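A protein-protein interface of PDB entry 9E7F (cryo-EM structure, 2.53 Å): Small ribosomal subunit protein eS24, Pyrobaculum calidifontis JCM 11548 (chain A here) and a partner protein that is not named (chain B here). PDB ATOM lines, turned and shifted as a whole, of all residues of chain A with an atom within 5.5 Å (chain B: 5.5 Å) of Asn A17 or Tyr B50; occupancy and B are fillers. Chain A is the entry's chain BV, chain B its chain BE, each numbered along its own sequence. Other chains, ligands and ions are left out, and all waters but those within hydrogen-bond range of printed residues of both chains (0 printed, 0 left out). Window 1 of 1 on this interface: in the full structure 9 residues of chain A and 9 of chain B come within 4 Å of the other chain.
Asn A17 touches just one residue of chain B: Tyr B50.
Tyr B50 touches just these residues of chain A: Arg A15 (3.5 Å), Asn A17 (3.1 Å), Leu A19 (3.4 Å) and Leu A20 (3.5 Å).
Of the printed residues of chain A, Ile B60 touches Leu A19 (3.9 Å) and Leu A20 (3.9 Å).
Printed residues of chain A within 4 Å of Lys B52: Glu A24 (3.4 Å).
Of the printed residues of chain B, Leu A19 touches Tyr B50, Ile B60 and Ile B88.
Glu A16 touches none of the printed residues of chain B.
The nearest residue of chain B that does not touch Asn A17 is Ile B60 (5.3 Å).
The nearest residue of chain A that does not touch Tyr B50 is Glu A24 (4.4 Å).
NH2 of Arg A15 touches O of Arg B49 (3.5 Å).
Tyr B50 touches Arg A15.
CD1 of Leu A19 touches CG of Tyr B50 (3.4 Å).
CG2 of Ile B60 touches CD1 of Leu A19, 3.9 Å away.
Ile B88 touches Leu A19 (CG2 to CD2, 3.7 Å).
Tyr B50 touches Leu A20.
CG of Leu A20 touches CD1 of Ile B60, 3.9 Å away.
Hydrophobic or aromatic side chains of chain B within 4 Å of the printed part of chain A: Tyr B50, Ile B60 and Ile B88.
Among the printed residues, Asp or Glu carboxylates within 4 Å of a Lys or Arg side-chain nitrogen of the other chain: Glu A24 with Lys B52.
O of Tyr B50 is in hydrogen-bond range of ND2 of Asn A17, at 3.4 Å.
The side-chain amino group of Lys B52 lies within salt-bridge range of the side-chain carboxylate of Glu A24 (3.4 Å).
NZ of Lys B52 sits at hydrogen-bond distance from O of Arg B49, 2.6 Å away.
The backbone carbonyl oxygen of Glu B93 sits at hydrogen-bond distance from the backbone NH of Ile B88, 3.0 Å away.
NE of Arg A15 lies within salt-bridge range of OE1 of Glu A24.
The side-chain amide oxygen (OD1) of Asn A17 sits at hydrogen-bond distance from the backbone NH (N) of Leu A19, 3.0 Å away.
N of Asn A17 is in hydrogen-bond range of O of Arg A22 (2.9 Å).
The guanidinium group of Arg A22 lies within salt-bridge range of the side-chain carboxylate of Glu A24, 3.0 Å away.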
ATOM      1  N   ARG A  15      11.912  26.828  18.641  1.00  0.00           N
ATOM      2  CA  ARG A  15      12.202  25.665  19.468  1.00  0.00           C
ATOM      3  C   ARG A  15      11.008  25.364  20.358  1.00  0.00           C
ATOM      4  O   ARG A  15      10.520  26.246  21.070  1.00  0.00           O
ATOM      5  CB  ARG A  15      13.448  25.887  20.323  1.00  0.00           C
ATOM      6  CG  ARG A  15      14.013  24.615  20.916  1.00  0.00           C
ATOM      7  CD  ARG A  15      15.137  24.923  21.878  1.00  0.00           C
ATOM      8  NE  ARG A  15      14.625  25.290  23.191  1.00  0.00           N
ATOM      9  CZ  ARG A  15      14.328  24.423  24.150  1.00  0.00           C
ATOM     10  NH1 ARG A  15      14.494  23.121  23.981  1.00  0.00           N
ATOM     11  NH2 ARG A  15      13.852  24.873  25.307  1.00  0.00           N
ATOM     12  N   GLU A  16      10.552  24.119  20.326  1.00  0.00           N
ATOM     13  CA  GLU A  16       9.378  23.689  21.074  1.00  0.00           C
ATOM     14  C   GLU A  16       9.819  23.211  22.449  1.00  0.00           C
ATOM     15  O   GLU A  16      10.557  22.229  22.564  1.00  0.00           O
ATOM     16  CB  GLU A  16       8.632  22.590  20.321  1.00  0.00           C
ATOM     17  CG  GLU A  16       7.213  22.310  20.812  1.00  0.00           C
ATOM     18  CD  GLU A  16       6.413  23.558  21.138  1.00  0.00           C
ATOM     19  OE1 GLU A  16       5.546  23.485  22.035  1.00  0.00           O
ATOM     20  OE2 GLU A  16       6.612  24.597  20.478  1.00  0.00           O
ATOM     21  N   ASN A  17       9.359  23.899  23.486  1.00  0.00           N
ATOM     22  CA  ASN A  17       9.677  23.564  24.868  1.00  0.00           C
ATOM     23  C   ASN A  17       8.387  23.142  25.559  1.00  0.00           C
ATOM     24  O   ASN A  17       7.508  23.972  25.810  1.00  0.00           O
ATOM     25  CB  ASN A  17      10.336  24.750  25.568  1.00  0.00           C
ATOM     26  CG  ASN A  17      10.677  24.467  27.016  1.00  0.00           C
ATOM     27  OD1 ASN A  17      10.667  23.322  27.464  1.00  0.00           O
ATOM     28  ND2 ASN A  17      11.010  25.516  27.752  1.00  0.00           N
ATOM     29  N   LYS A  18       8.281  21.849  25.865  1.00  0.00           N
ATOM     30  CA  LYS A  18       7.113  21.336  26.567  1.00  0.00           C
ATOM     31  C   LYS A  18       7.232  21.503  28.074  1.00  0.00           C
ATOM     32  O   LYS A  18       6.213  21.521  28.771  1.00  0.00           O
ATOM     33  CB  LYS A  18       6.904  19.863  26.231  1.00  0.00           C
ATOM     34  CG  LYS A  18       6.571  19.608  24.783  1.00  0.00           C
ATOM     35  CD  LYS A  18       5.087  19.784  24.532  1.00  0.00           C
ATOM     36  CE  LYS A  18       4.787  19.842  23.046  1.00  0.00           C
ATOM     37  NZ  LYS A  18       4.471  18.498  22.497  1.00  0.00           N
ATOM     38  N   LEU A  19       8.459  21.610  28.589  1.00  0.00           N
ATOM     39  CA  LEU A  19       8.654  21.728  30.028  1.00  0.00           C
ATOM     40  C   LEU A  19       8.089  23.038  30.552  1.00  0.00           C
ATOM     41  O   LEU A  19       7.331  23.056  31.527  1.00  0.00           O
ATOM     42  CB  LEU A  19      10.139  21.614  30.361  1.00  0.00           C
ATOM     43  CG  LEU A  19      10.787  20.251  30.137  1.00  0.00           C
ATOM     44  CD1 LEU A  19      12.267  20.324  30.417  1.00  0.00           C
ATOM     45  CD2 LEU A  19      10.143  19.230  31.029  1.00  0.00           C
ATOM     46  N   LEU A  20       8.442  24.147  29.916  1.00  0.00           N
ATOM     47  CA  LEU A  20       7.935  25.449  30.312  1.00  0.00           C
ATOM     48  C   LEU A  20       6.658  25.825  29.582  1.00  0.00           C
ATOM     49  O   LEU A  20       6.119  26.908  29.826  1.00  0.00           O
ATOM     50  CB  LEU A  20       9.000  26.519  30.080  1.00  0.00           C
ATOM     51  CG  LEU A  20      10.185  26.448  31.037  1.00  0.00           C
ATOM     52  CD1 LEU A  20      11.343  27.260  30.513  1.00  0.00           C
ATOM     53  CD2 LEU A  20       9.769  26.943  32.401  1.00  0.00           C
ATOM     54  N   GLY A  21       6.160  24.957  28.707  1.00  0.00           N
ATOM     55  CA  GLY A  21       4.924  25.211  28.000  1.00  0.00           C
ATOM     56  C   GLY A  21       5.007  26.406  27.082  1.00  0.00           C
ATOM     57  O   GLY A  21       4.102  27.245  27.067  1.00  0.00           O
ATOM     58  N   ARG A  22       6.089  26.503  26.316  1.00  0.00           N
ATOM     59  CA  ARG A  22       6.271  27.635  25.423  1.00  0.00           C
ATOM     60  C   ARG A  22       7.090  27.210  24.218  1.00  0.00           C
ATOM     61  O   ARG A  22       7.793  26.198  24.241  1.00  0.00           O
ATOM     62  CB  ARG A  22       6.958  28.799  26.133  1.00  0.00           C
ATOM     63  CG  ARG A  22       8.434  28.580  26.368  1.00  0.00           C
ATOM     64  CD  ARG A  22       8.917  29.411  27.525  1.00  0.00           C
ATOM     65  NE  ARG A  22      10.344  29.239  27.754  1.00  0.00           N
ATOM     66  CZ  ARG A  22      11.061  29.985  28.580  1.00  0.00           C
ATOM     67  NH1 ARG A  22      10.518  30.982  29.256  1.00  0.00           N
ATOM     68  NH2 ARG A  22      12.355  29.722  28.733  1.00  0.00           N
ATOM     69  N   LYS A  23       6.991  28.005  23.158  1.00  0.00           N
ATOM     70  CA  LYS A  23       7.785  27.819  21.950  1.00  0.00           C
ATOM     71  C   LYS A  23       8.672  29.043  21.780  1.00  0.00           C
ATOM     72  O   LYS A  23       8.222  30.079  21.282  1.00  0.00           O
ATOM     73  CB  LYS A  23       6.894  27.599  20.733  1.00  0.00           C
ATOM     74  CG  LYS A  23       5.621  28.417  20.736  1.00  0.00           C
ATOM     75  CD  LYS A  23       4.536  27.729  19.930  1.00  0.00           C
ATOM     76  CE  LYS A  23       5.101  27.138  18.655  1.00  0.00           C
ATOM     77  NZ  LYS A  23       4.185  26.128  18.067  1.00  0.00           N
ATOM     78  N   GLU A  24       9.925  28.920  22.202  1.00  0.00           N
ATOM     79  CA  GLU A  24      10.879  30.019  22.124  1.00  0.00           C
ATOM     80  C   GLU A  24      11.202  30.263  20.659  1.00  0.00           C
ATOM     81  O   GLU A  24      11.959  29.504  20.047  1.00  0.00           O
ATOM     82  CB  GLU A  24      12.131  29.681  22.924  1.00  0.00           C
ATOM     83  CG  GLU A  24      11.835  29.210  24.332  1.00  0.00           C
ATOM     84  CD  GLU A  24      12.951  28.361  24.901  1.00  0.00           C
ATOM     85  OE1 GLU A  24      13.589  27.625  24.123  1.00  0.00           O
ATOM     86  OE2 GLU A  24      13.193  28.432  26.125  1.00  0.00           O
ATOM     87  N   VAL B  44      19.814  20.899  33.195  1.00  0.00           N
ATOM     88  CA  VAL B  44      18.593  21.463  32.642  1.00  0.00           C
ATOM     89  C   VAL B  44      18.847  22.778  31.924  1.00  0.00           C
ATOM     90  O   VAL B  44      18.110  23.121  30.994  1.00  0.00           O
ATOM     91  CB  VAL B  44      17.548  21.644  33.756  1.00  0.00           C
ATOM     92  CG1 VAL B  44      16.248  22.171  33.186  1.00  0.00           C
ATOM     93  CG2 VAL B  44      17.320  20.332  34.469  1.00  0.00           C
ATOM     94  N   ARG B  45      19.863  23.531  32.327  1.00  0.00           N
ATOM     95  CA  ARG B  45      20.146  24.831  31.732  1.00  0.00           C
ATOM     96  C   ARG B  45      21.209  24.797  30.649  1.00  0.00           C
ATOM     97  O   ARG B  45      21.116  25.553  29.684  1.00  0.00           O
ATOM     98  CB  ARG B  45      20.576  25.828  32.810  1.00  0.00           C
ATOM     99  CG  ARG B  45      20.853  27.202  32.248  1.00  0.00           C
ATOM    100  CD  ARG B  45      21.251  28.189  33.316  1.00  0.00           C
ATOM    101  NE  ARG B  45      22.239  27.642  34.232  1.00  0.00           N
ATOM    102  CZ  ARG B  45      22.624  28.241  35.349  1.00  0.00           C
ATOM    103  NH1 ARG B  45      22.144  29.421  35.697  1.00  0.00           N
ATOM    104  NH2 ARG B  45      23.514  27.642  36.134  1.00  0.00           N
ATOM    105  N   LEU B  48      20.844  20.401  28.300  1.00  0.00           N
ATOM    106  CA  LEU B  48      19.590  20.285  27.575  1.00  0.00           C
ATOM    107  C   LEU B  48      19.049  21.625  27.108  1.00  0.00           C
ATOM    108  O   LEU B  48      18.203  21.649  26.212  1.00  0.00           O
ATOM    109  CB  LEU B  48      18.536  19.583  28.437  1.00  0.00           C
ATOM    110  CG  LEU B  48      18.935  18.184  28.888  1.00  0.00           C
ATOM    111  CD1 LEU B  48      17.856  17.570  29.755  1.00  0.00           C
ATOM    112  CD2 LEU B  48      19.223  17.312  27.688  1.00  0.00           C
ATOM    113  N   ARG B  49      19.505  22.729  27.694  1.00  0.00           N
ATOM    114  CA  ARG B  49      19.133  24.080  27.271  1.00  0.00           C
ATOM    115  C   ARG B  49      17.642  24.350  27.429  1.00  0.00           C
ATOM    116  O   ARG B  49      17.082  25.197  26.730  1.00  0.00           O
ATOM    117  CB  ARG B  49      19.564  24.347  25.827  1.00  0.00           C
ATOM    118  CG  ARG B  49      21.051  24.568  25.653  1.00  0.00           C
ATOM    119  CD  ARG B  49      21.430  24.620  24.189  1.00  0.00           C
ATOM    120  NE  ARG B  49      21.643  23.295  23.618  1.00  0.00           N
ATOM    121  CZ  ARG B  49      20.698  22.549  23.062  1.00  0.00           C
ATOM    122  NH1 ARG B  49      19.446  22.963  22.981  1.00  0.00           N
ATOM    123  NH2 ARG B  49      21.020  21.357  22.570  1.00  0.00           N
ATOM    124  N   TYR B  50      16.979  23.643  28.341  1.00  0.00           N
ATOM    125  CA  TYR B  50      15.548  23.827  28.516  1.00  0.00           C
ATOM    126  C   TYR B  50      15.214  25.049  29.354  1.00  0.00           C
ATOM    127  O   TYR B  50      14.083  25.535  29.289  1.00  0.00           O
ATOM    128  CB  TYR B  50      14.938  22.578  29.149  1.00  0.00           C
ATOM    129  CG  TYR B  50      14.421  21.588  28.137  1.00  0.00           C
ATOM    130  CD1 TYR B  50      13.408  21.936  27.262  1.00  0.00           C
ATOM    131  CD2 TYR B  50      14.945  20.309  28.054  1.00  0.00           C
ATOM    132  CE1 TYR B  50      12.929  21.044  26.333  1.00  0.00           C
ATOM    133  CE2 TYR B  50      14.473  19.405  27.125  1.00  0.00           C
ATOM    134  CZ  TYR B  50      13.462  19.781  26.265  1.00  0.00           C
ATOM    135  OH  TYR B  50      12.979  18.893  25.334  1.00  0.00           O
ATOM    136  N   ALA B  51      16.168  25.556  30.127  1.00  0.00           N
ATOM    137  CA  ALA B  51      15.966  26.714  30.981  1.00  0.00           C
ATOM    138  C   ALA B  51      17.010  27.768  30.657  1.00  0.00           C
ATOM    139  O   ALA B  51      18.185  27.449  30.457  1.00  0.00           O
ATOM    140  CB  ALA B  51      16.051  26.331  32.456  1.00  0.00           C
ATOM    141  N   LYS B  52      16.578  29.022  30.607  1.00  0.00           N
ATOM    142  CA  LYS B  52      17.471  30.122  30.277  1.00  0.00           C
ATOM    143  C   LYS B  52      18.092  30.778  31.498  1.00  0.00           C
ATOM    144  O   LYS B  52      19.100  31.475  31.356  1.00  0.00           O
ATOM    145  CB  LYS B  52      16.722  31.182  29.462  1.00  0.00           C
ATOM    146  CG  LYS B  52      16.369  30.733  28.060  1.00  0.00           C
ATOM    147  CD  LYS B  52      17.498  29.925  27.445  1.00  0.00           C
ATOM    148  CE  LYS B  52      17.024  29.109  26.250  1.00  0.00           C
ATOM    149  NZ  LYS B  52      16.534  27.754  26.636  1.00  0.00           N
ATOM    150  N   ILE B  60      11.541  24.134  36.641  1.00  0.00           N
ATOM    151  CA  ILE B  60      11.347  22.880  35.919  1.00  0.00           C
ATOM    152  C   ILE B  60      11.590  21.703  36.842  1.00  0.00           C
ATOM    153  O   ILE B  60      10.850  20.715  36.834  1.00  0.00           O
ATOM    154  CB  ILE B  60      12.274  22.817  34.697  1.00  0.00           C
ATOM    155  CG1 ILE B  60      11.781  23.759  33.603  1.00  0.00           C
ATOM    156  CG2 ILE B  60      12.373  21.395  34.200  1.00  0.00           C
ATOM    157  CD1 ILE B  60      12.796  24.000  32.522  1.00  0.00           C
ATOM    158  N   ILE B  88      13.087  12.570  31.256  1.00  0.00           N
ATOM    159  CA  ILE B  88      12.261  13.772  31.270  1.00  0.00           C
ATOM    160  C   ILE B  88      10.823  13.339  31.035  1.00  0.00           C
ATOM    161  O   ILE B  88      10.465  12.921  29.928  1.00  0.00           O
ATOM    162  CB  ILE B  88      12.717  14.787  30.218  1.00  0.00           C
ATOM    163  CG1 ILE B  88      14.157  15.212  30.490  1.00  0.00           C
ATOM    164  CG2 ILE B  88      11.798  15.982  30.216  1.00  0.00           C
ATOM    165  CD1 ILE B  88      14.665  16.256  29.542  1.00  0.00           C
ATOM    166  N   THR B  91       8.232  14.923  28.229  1.00  0.00           N
ATOM    167  CA  THR B  91       8.664  14.699  26.859  1.00  0.00           C
ATOM    168  C   THR B  91       8.984  13.243  26.556  1.00  0.00           C
ATOM    169  O   THR B  91       9.005  12.865  25.382  1.00  0.00           O
ATOM    170  CB  THR B  91       9.899  15.552  26.542  1.00  0.00           C
ATOM    171  OG1 THR B  91       9.695  16.878  27.039  1.00  0.00           O
ATOM    172  CG2 THR B  91      10.118  15.624  25.049  1.00  0.00           C
ATOM    173  N   GLU B  93      11.791  11.602  26.851  1.00  0.00           N
ATOM    174  CA  GLU B  93      13.146  11.307  26.412  1.00  0.00           C
ATOM    175  C   GLU B  93      13.973  10.744  27.560  1.00  0.00           C
ATOM    176  O   GLU B  93      13.794  11.127  28.718  1.00  0.00           O
ATOM    177  CB  GLU B  93      13.811  12.561  25.852  1.00  0.00           C
ATOM    178  CG  GLU B  93      13.397  13.841  26.529  1.00  0.00           C
ATOM    179  CD  GLU B  93      13.819  15.062  25.742  1.00  0.00           C
ATOM    180  OE1 GLU B  93      14.953  15.063  25.222  1.00  0.00           O
ATOM    181  OE2 GLU B  93      13.030  16.023  25.646  1.00  0.00           O
